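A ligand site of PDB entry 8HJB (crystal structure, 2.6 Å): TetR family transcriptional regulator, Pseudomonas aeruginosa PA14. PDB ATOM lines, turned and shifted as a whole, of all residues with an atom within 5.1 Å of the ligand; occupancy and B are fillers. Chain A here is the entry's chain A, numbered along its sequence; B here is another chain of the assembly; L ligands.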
ATOM      1  N   TYR A  92      27.336   4.159  24.962  1.00  0.00           N
ATOM      2  CA  TYR A  92      26.558   5.347  25.312  1.00  0.00           C
ATOM      3  C   TYR A  92      25.571   5.047  26.436  1.00  0.00           C
ATOM      4  O   TYR A  92      25.427   5.847  27.370  1.00  0.00           O
ATOM      5  CB  TYR A  92      25.831   5.874  24.075  1.00  0.00           C
ATOM      6  CG  TYR A  92      24.770   6.914  24.384  1.00  0.00           C
ATOM      7  CD1 TYR A  92      25.121   8.212  24.726  1.00  0.00           C
ATOM      8  CD2 TYR A  92      23.424   6.590  24.329  1.00  0.00           C
ATOM      9  CE1 TYR A  92      24.159   9.167  25.008  1.00  0.00           C
ATOM     10  CE2 TYR A  92      22.453   7.535  24.609  1.00  0.00           C
ATOM     11  CZ  TYR A  92      22.826   8.823  24.944  1.00  0.00           C
ATOM     12  OH  TYR A  92      21.864   9.768  25.225  1.00  0.00           O
ATOM     13  N   ARG A  96      25.165   6.472  30.525  1.00  0.00           N
ATOM     14  CA  ARG A  96      23.982   7.094  31.104  1.00  0.00           C
ATOM     15  C   ARG A  96      23.420   6.276  32.257  1.00  0.00           C
ATOM     16  O   ARG A  96      22.954   6.842  33.251  1.00  0.00           O
ATOM     17  CB  ARG A  96      22.909   7.282  30.018  1.00  0.00           C
ATOM     18  CG  ARG A  96      23.433   7.865  28.722  1.00  0.00           C
ATOM     19  CD  ARG A  96      23.058   9.322  28.571  1.00  0.00           C
ATOM     20  NE  ARG A  96      21.638   9.490  28.254  1.00  0.00           N
ATOM     21  CZ  ARG A  96      20.916  10.540  28.596  1.00  0.00           C
ATOM     22  NH1 ARG A  96      21.433  11.545  29.289  1.00  0.00           N
ATOM     23  NH2 ARG A  96      19.627  10.593  28.247  1.00  0.00           N
ATOM     24  N   TYR A 103      22.971  10.617  38.132  1.00  0.00           N
ATOM     25  CA  TYR A 103      21.924  11.174  37.296  1.00  0.00           C
ATOM     26  C   TYR A 103      20.893  11.919  38.134  1.00  0.00           C
ATOM     27  O   TYR A 103      20.518  13.054  37.812  1.00  0.00           O
ATOM     28  CB  TYR A 103      21.259  10.049  36.487  1.00  0.00           C
ATOM     29  CG  TYR A 103      20.126  10.486  35.578  1.00  0.00           C
ATOM     30  CD1 TYR A 103      18.841  10.639  36.060  1.00  0.00           C
ATOM     31  CD2 TYR A 103      20.353  10.722  34.227  1.00  0.00           C
ATOM     32  CE1 TYR A 103      17.807  11.035  35.227  1.00  0.00           C
ATOM     33  CE2 TYR A 103      19.331  11.119  33.387  1.00  0.00           C
ATOM     34  CZ  TYR A 103      18.052  11.271  33.890  1.00  0.00           C
ATOM     35  OH  TYR A 103      17.028  11.657  33.059  1.00  0.00           O
ATOM     36  N   ASP A 107      19.958  15.745  38.103  1.00  0.00           N
ATOM     37  CA  ASP A 107      18.558  16.079  37.871  1.00  0.00           C
ATOM     38  C   ASP A 107      18.080  17.125  38.869  1.00  0.00           C
ATOM     39  O   ASP A 107      17.435  18.114  38.489  1.00  0.00           O
ATOM     40  CB  ASP A 107      17.711  14.804  37.947  1.00  0.00           C
ATOM     41  CG  ASP A 107      16.285  15.011  37.438  1.00  0.00           C
ATOM     42  OD1 ASP A 107      15.881  16.160  37.214  1.00  0.00           O
ATOM     43  OD2 ASP A 107      15.578  13.993  37.270  1.00  0.00           O
ATOM     44  N   GLU A 110      19.875  20.383  38.256  1.00  0.00           N
ATOM     45  CA  GLU A 110      19.398  21.087  37.065  1.00  0.00           C
ATOM     46  C   GLU A 110      18.441  22.219  37.409  1.00  0.00           C
ATOM     47  O   GLU A 110      18.326  23.175  36.646  1.00  0.00           O
ATOM     48  CB  GLU A 110      18.727  20.110  36.111  1.00  0.00           C
ATOM     49  CG  GLU A 110      18.371  20.677  34.732  1.00  0.00           C
ATOM     50  CD  GLU A 110      19.586  21.138  33.945  1.00  0.00           C
ATOM     51  OE1 GLU A 110      20.713  20.671  34.241  1.00  0.00           O
ATOM     52  OE2 GLU A 110      19.421  21.979  33.034  1.00  0.00           O
ATOM     53  N   GLU A 111      17.750  22.139  38.549  1.00  0.00           N
ATOM     54  CA  GLU A 111      16.795  23.168  38.948  1.00  0.00           C
ATOM     55  C   GLU A 111      17.402  24.226  39.854  1.00  0.00           C
ATOM     56  O   GLU A 111      16.807  25.300  40.008  1.00  0.00           O
ATOM     57  CB  GLU A 111      15.599  22.521  39.657  1.00  0.00           C
ATOM     58  CG  GLU A 111      15.300  21.100  39.216  1.00  0.00           C
ATOM     59  CD  GLU A 111      14.675  21.047  37.833  1.00  0.00           C
ATOM     60  OE1 GLU A 111      13.659  21.744  37.622  1.00  0.00           O
ATOM     61  OE2 GLU A 111      15.191  20.326  36.972  1.00  0.00           O
ATOM     62  N   ARG A 130      26.411  20.474  26.031  1.00  0.00           N
ATOM     63  CA  ARG A 130      25.219  19.636  25.935  1.00  0.00           C
ATOM     64  C   ARG A 130      24.694  19.629  24.503  1.00  0.00           C
ATOM     65  O   ARG A 130      24.252  18.576  24.015  1.00  0.00           O
ATOM     66  CB  ARG A 130      24.131  20.132  26.891  1.00  0.00           C
ATOM     67  CG  ARG A 130      24.590  20.297  28.331  1.00  0.00           C
ATOM     68  CD  ARG A 130      23.506  19.919  29.330  1.00  0.00           C
ATOM     69  NE  ARG A 130      24.090  19.339  30.527  1.00  0.00           N
ATOM     70  CZ  ARG A 130      23.389  18.971  31.598  1.00  0.00           C
ATOM     71  NH1 ARG A 130      22.076  19.104  31.636  1.00  0.00           N
ATOM     72  NH2 ARG A 130      24.020  18.450  32.644  1.00  0.00           N
ATOM     73  N   PHE A 134      24.623  16.704  22.237  1.00  0.00           N
ATOM     74  CA  PHE A 134      23.352  16.413  21.566  1.00  0.00           C
ATOM     75  C   PHE A 134      23.556  16.244  20.066  1.00  0.00           C
ATOM     76  O   PHE A 134      22.938  15.361  19.464  1.00  0.00           O
ATOM     77  CB  PHE A 134      22.329  17.517  21.824  1.00  0.00           C
ATOM     78  CG  PHE A 134      20.959  17.185  21.306  1.00  0.00           C
ATOM     79  CD1 PHE A 134      20.412  15.924  21.510  1.00  0.00           C
ATOM     80  CD2 PHE A 134      20.225  18.117  20.590  1.00  0.00           C
ATOM     81  CE1 PHE A 134      19.158  15.614  21.025  1.00  0.00           C
ATOM     82  CE2 PHE A 134      18.970  17.808  20.104  1.00  0.00           C
ATOM     83  CZ  PHE A 134      18.442  16.556  20.323  1.00  0.00           C
ATOM     84  N   LEU A 137      24.986  12.826  18.868  1.00  0.00           N
ATOM     85  CA  LEU A 137      24.148  11.647  19.043  1.00  0.00           C
ATOM     86  C   LEU A 137      23.366  11.312  17.778  1.00  0.00           C
ATOM     87  O   LEU A 137      23.404  10.175  17.293  1.00  0.00           O
ATOM     88  CB  LEU A 137      23.199  11.856  20.222  1.00  0.00           C
ATOM     89  CG  LEU A 137      22.268  10.712  20.616  1.00  0.00           C
ATOM     90  CD1 LEU A 137      23.041   9.400  20.738  1.00  0.00           C
ATOM     91  CD2 LEU A 137      21.549  11.044  21.907  1.00  0.00           C
ATOM     92  N   TYR A 159      16.370   9.243  19.700  1.00  0.00           N
ATOM     93  CA  TYR A 159      17.016   9.756  20.908  1.00  0.00           C
ATOM     94  C   TYR A 159      16.020  10.139  21.987  1.00  0.00           C
ATOM     95  O   TYR A 159      16.409  10.295  23.148  1.00  0.00           O
ATOM     96  CB  TYR A 159      17.938  10.937  20.555  1.00  0.00           C
ATOM     97  CG  TYR A 159      17.316  12.198  19.960  1.00  0.00           C
ATOM     98  CD1 TYR A 159      16.258  12.852  20.574  1.00  0.00           C
ATOM     99  CD2 TYR A 159      17.809  12.734  18.778  1.00  0.00           C
ATOM    100  CE1 TYR A 159      15.711  14.003  20.027  1.00  0.00           C
ATOM    101  CE2 TYR A 159      17.264  13.875  18.221  1.00  0.00           C
ATOM    102  CZ  TYR A 159      16.215  14.510  18.846  1.00  0.00           C
ATOM    103  OH  TYR A 159      15.669  15.640  18.298  1.00  0.00           O
ATOM    104  N   CYS A 160      14.738  10.303  21.635  1.00  0.00           N
ATOM    105  CA  CYS A 160      13.716  10.467  22.666  1.00  0.00           C
ATOM    106  C   CYS A 160      13.427   9.141  23.353  1.00  0.00           C
ATOM    107  O   CYS A 160      13.310   9.086  24.581  1.00  0.00           O
ATOM    108  CB  CYS A 160      12.441  11.044  22.064  1.00  0.00           C
ATOM    109  SG  CYS A 160      12.553  12.811  21.664  1.00  0.00           S
ATOM    110  N   TRP A 163      16.367   8.430  25.572  1.00  0.00           N
ATOM    111  CA  TRP A 163      16.267   9.207  26.810  1.00  0.00           C
ATOM    112  C   TRP A 163      15.140   8.694  27.681  1.00  0.00           C
ATOM    113  O   TRP A 163      15.275   8.647  28.916  1.00  0.00           O
ATOM    114  CB  TRP A 163      16.069  10.689  26.479  1.00  0.00           C
ATOM    115  CG  TRP A 163      15.940  11.566  27.696  1.00  0.00           C
ATOM    116  CD1 TRP A 163      16.945  12.240  28.329  1.00  0.00           C
ATOM    117  CD2 TRP A 163      14.738  11.849  28.425  1.00  0.00           C
ATOM    118  NE1 TRP A 163      16.440  12.931  29.404  1.00  0.00           N
ATOM    119  CE2 TRP A 163      15.087  12.700  29.486  1.00  0.00           C
ATOM    120  CE3 TRP A 163      13.411  11.460  28.279  1.00  0.00           C
ATOM    121  CZ2 TRP A 163      14.151  13.174  30.397  1.00  0.00           C
ATOM    122  CZ3 TRP A 163      12.477  11.934  29.180  1.00  0.00           C
ATOM    123  CH2 TRP A 163      12.850  12.777  30.224  1.00  0.00           C
ATOM    124  N   HIS A 167      16.011   7.500  31.546  1.00  0.00           N
ATOM    125  CA  HIS A 167      15.300   8.256  32.577  1.00  0.00           C
ATOM    126  C   HIS A 167      14.404   7.342  33.408  1.00  0.00           C
ATOM    127  O   HIS A 167      14.294   7.519  34.620  1.00  0.00           O
ATOM    128  CB  HIS A 167      14.478   9.382  31.926  1.00  0.00           C
ATOM    129  CG  HIS A 167      13.923  10.366  32.907  1.00  0.00           C
ATOM    130  ND1 HIS A 167      14.723  11.113  33.750  1.00  0.00           N
ATOM    131  CD2 HIS A 167      12.653  10.750  33.171  1.00  0.00           C
ATOM    132  CE1 HIS A 167      13.965  11.902  34.488  1.00  0.00           C
ATOM    133  NE2 HIS A 167      12.698  11.694  34.159  1.00  0.00           N
ATOM    134  N   ARG B 104       0.690  10.487  35.450  1.00  0.00           N
ATOM    135  CA  ARG B 104       1.373  11.557  36.167  1.00  0.00           C
ATOM    136  C   ARG B 104       0.539  12.030  37.352  1.00  0.00           C
ATOM    137  O   ARG B 104       1.083  12.316  38.427  1.00  0.00           O
ATOM    138  CB  ARG B 104       1.665  12.726  35.217  1.00  0.00           C
ATOM    139  CG  ARG B 104       2.524  13.828  35.806  1.00  0.00           C
ATOM    140  CD  ARG B 104       3.855  13.277  36.329  1.00  0.00           C
ATOM    141  NE  ARG B 104       4.998  14.022  35.830  1.00  0.00           N
ATOM    142  CZ  ARG B 104       5.237  15.301  36.068  1.00  0.00           C
ATOM    143  NH1 ARG B 104       4.444  16.027  36.837  1.00  0.00           N
ATOM    144  NH2 ARG B 104       6.304  15.876  35.515  1.00  0.00           N
ATOM    145  N   ALA B 171       7.371  10.806  31.426  1.00  0.00           N
ATOM    146  CA  ALA B 171       8.264  11.901  31.786  1.00  0.00           C
ATOM    147  C   ALA B 171       8.794  12.601  30.549  1.00  0.00           C
ATOM    148  O   ALA B 171       9.092  13.802  30.590  1.00  0.00           O
ATOM    149  CB  ALA B 171       9.418  11.377  32.644  1.00  0.00           C
ATOM    150  N   LEU B 172       8.930  11.870  29.433  1.00  0.00           N
ATOM    151  CA  LEU B 172       9.215  12.514  28.157  1.00  0.00           C
ATOM    152  C   LEU B 172       8.004  13.308  27.670  1.00  0.00           C
ATOM    153  O   LEU B 172       8.148  14.384  27.085  1.00  0.00           O
ATOM    154  CB  LEU B 172       9.620  11.468  27.114  1.00  0.00           C
ATOM    155  CG  LEU B 172       9.786  11.946  25.674  1.00  0.00           C
ATOM    156  CD1 LEU B 172      11.228  12.311  25.373  1.00  0.00           C
ATOM    157  CD2 LEU B 172       9.272  10.895  24.704  1.00  0.00           C
ATOM    158  N   SER B 175       8.139  16.737  29.528  1.00  0.00           N
ATOM    159  CA  SER B 175       9.288  17.624  29.415  1.00  0.00           C
ATOM    160  C   SER B 175       8.944  18.827  28.542  1.00  0.00           C
ATOM    161  O   SER B 175       7.955  18.800  27.796  1.00  0.00           O
ATOM    162  CB  SER B 175      10.479  16.863  28.809  1.00  0.00           C
ATOM    163  OG  SER B 175      10.992  15.913  29.728  1.00  0.00           O
ATOM    164  N   PRO B 176       9.737  19.903  28.618  1.00  0.00           N
ATOM    165  CA  PRO B 176       9.506  21.060  27.743  1.00  0.00           C
ATOM    166  C   PRO B 176       9.569  20.736  26.259  1.00  0.00           C
ATOM    167  O   PRO B 176       9.422  21.614  25.405  1.00  0.00           O
ATOM    168  CB  PRO B 176      10.639  22.021  28.140  1.00  0.00           C
ATOM    169  CG  PRO B 176      10.886  21.708  29.575  1.00  0.00           C
ATOM    170  CD  PRO B 176      10.685  20.222  29.709  1.00  0.00           C
ATOM    171  N   PHE B 177       9.794  19.457  25.934  1.00  0.00           N
ATOM    172  CA  PHE B 177       9.816  18.934  24.584  1.00  0.00           C
ATOM    173  C   PHE B 177       8.420  18.622  24.042  1.00  0.00           C
ATOM    174  O   PHE B 177       8.310  18.175  22.896  1.00  0.00           O
ATOM    175  CB  PHE B 177      10.667  17.662  24.560  1.00  0.00           C
ATOM    176  CG  PHE B 177      11.476  17.461  23.313  1.00  0.00           C
ATOM    177  CD1 PHE B 177      10.926  16.826  22.208  1.00  0.00           C
ATOM    178  CD2 PHE B 177      12.791  17.890  23.246  1.00  0.00           C
ATOM    179  CE1 PHE B 177      11.666  16.648  21.052  1.00  0.00           C
ATOM    180  CE2 PHE B 177      13.539  17.712  22.102  1.00  0.00           C
ATOM    181  CZ  PHE B 177      12.977  17.086  21.005  1.00  0.00           C
HETATM  182  N1  LIG L   1      19.612  13.399  25.406  1.00  0.00           N
HETATM  183  C1  LIG L   1      19.469  14.404  26.251  1.00  0.00           C
HETATM  184  N2  LIG L   1      18.324  15.071  26.350  1.00  0.00           N
HETATM  185  C2  LIG L   1      17.292  14.752  25.600  1.00  0.00           C
HETATM  186  C3  LIG L   1      17.395  13.708  24.705  1.00  0.00           C
HETATM  187  C4  LIG L   1      18.629  13.023  24.622  1.00  0.00           C
HETATM  188  N3  LIG L   1      18.812  11.904  23.686  1.00  0.00           N
HETATM  189  N4  LIG L   1      16.232  13.599  24.085  1.00  0.00           N
HETATM  190  C5  LIG L   1      15.414  14.538  24.576  1.00  0.00           C
HETATM  191  N5  LIG L   1      16.032  15.226  25.474  1.00  0.00           N
HETATM  192  C6  LIG L   1      15.446  16.341  26.222  1.00  0.00           C
HETATM  193  C7  LIG L   1      14.571  15.917  27.094  1.00  0.00           C
HETATM  194  O1  LIG L   1      13.309  15.644  26.477  1.00  0.00           O
HETATM  195  C8  LIG L   1      14.432  17.212  28.149  1.00  0.00           C
HETATM  196  O2  LIG L   1      13.612  18.235  27.555  1.00  0.00           O
HETATM  197  P1  LIG L   1      14.310  19.621  26.958  1.00  0.00           P
HETATM  198  O3  LIG L   1      15.427  19.264  26.046  1.00  0.00           O
HETATM  199  O4  LIG L   1      14.832  20.445  28.079  1.00  0.00           O
HETATM  200  O5  LIG L   1      13.283  20.405  26.199  1.00  0.00           O
HETATM  201  C9  LIG L   1      15.628  17.625  28.334  1.00  0.00           C
HETATM  202  O6  LIG L   1      16.495  17.055  27.099  1.00  0.00           O
HETATM  203  C10 LIG L   1      16.134  17.065  29.671  1.00  0.00           C
HETATM  204  O7  LIG L   1      17.563  16.833  29.680  1.00  0.00           O
HETATM  205  P2  LIG L   1      18.510  17.668  30.871  1.00  0.00           P
HETATM  206  O8  LIG L   1      19.862  18.044  30.288  1.00  0.00           O
HETATM  207  O9  LIG L   1      17.798  18.907  31.245  1.00  0.00           O
HETATM  208  O10 LIG L   1      18.750  16.765  32.260  1.00  0.00           O
HETATM  209  P3  LIG L   1      18.626  15.130  32.431  1.00  0.00           P
HETATM  210  O11 LIG L   1      18.727  14.457  31.118  1.00  0.00           O
HETATM  211  O12 LIG L   1      19.779  14.633  33.351  1.00  0.00           O
HETATM  212  O13 LIG L   1      17.207  14.754  33.154  1.00  0.00           O
HETATM  213  C11 LIG L   1      15.204  16.083  33.456  1.00  0.00           C
HETATM  214  C12 LIG L   1      16.014  15.115  32.524  1.00  0.00           C
HETATM  215  C13 LIG L   1      16.171  17.014  34.147  1.00  0.00           C
HETATM  216  C14 LIG L   1      14.463  15.286  34.476  1.00  0.00           C
HETATM  217  C15 LIG L   1      14.201  16.922  32.614  1.00  0.00           C
HETATM  218  O14 LIG L   1      13.707  16.157  31.552  1.00  0.00           O
HETATM  219  C16 LIG L   1      13.113  17.542  33.505  1.00  0.00           C
HETATM  220  O15 LIG L   1      13.390  18.503  34.120  1.00  0.00           O
HETATM  221  N6  LIG L   1      11.743  17.026  33.659  1.00  0.00           N
HETATM  222  C17 LIG L   1      11.174  15.837  32.997  1.00  0.00           C
HETATM  223  C18 LIG L   1      10.127  15.156  33.895  1.00  0.00           C
HETATM  224  C19 LIG L   1      10.763  14.429  35.052  1.00  0.00           C
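The guanidinium group (NH1) of Arg 130 is in salt-bridge range of an oxygen (O8) of the ligand (2.8 Å).
O of Tyr 159 is in hydrogen-bond range of N3 of the ligand (2.9 Å).
OH of Tyr 103 lies within hydrogen-bond range of O13 of the ligand (3.1 Å).
The indole nitrogen (NE1) of Trp 163 lies within hydrogen-bond range of an oxygen (O11) of the ligand, 3.2 Å away.
O14 of the ligand lies close to OG of Ser 175 of chain B, 3.3 Å away.
The guanidinium group (NH1) of Arg 130 lies within salt-bridge range of the side-chain carboxylate (OE1) of Glu 110 (3.3 Å).
OH of Tyr 103 lies within hydrogen-bond range of ND1 of His 167.
The backbone carbonyl oxygen (O) of Ala 171 of chain B lies within hydrogen-bond range of the side-chain hydroxyl (OG) of Ser 175 of chain B, 3.0 Å away.
The guanidinium group of Arg 96 is in hydrogen-bond range of the side-chain hydroxyl of Tyr 92 (3.1 Å).
Residues that only touch the ligand: Asp 107, Leu 137, His 167, Phe 177 of chain B, Pro 176 of chain B, Ala 171 of chain B, Glu 111, Glu 110 and Arg 96.
Hydrophobic or aromatic side chains that line the ligand: Tyr 103, Leu 137, Tyr 159, Trp 163, His 167, Pro 176 of chain B and Phe 177 of chain B.
Within 4 Å of the ligand: Arg 96, Tyr 103, Asp 107, Glu 110, Glu 111, Arg 130, Leu 137, Tyr 159, Trp 163, His 167, Ala 171 of chain B, Ser 175 of chain B, Pro 176 of chain B and Phe 177 of chain B.
The nearest printed residue that does not touch the ligand is Tyr 92 (4.03 Å).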
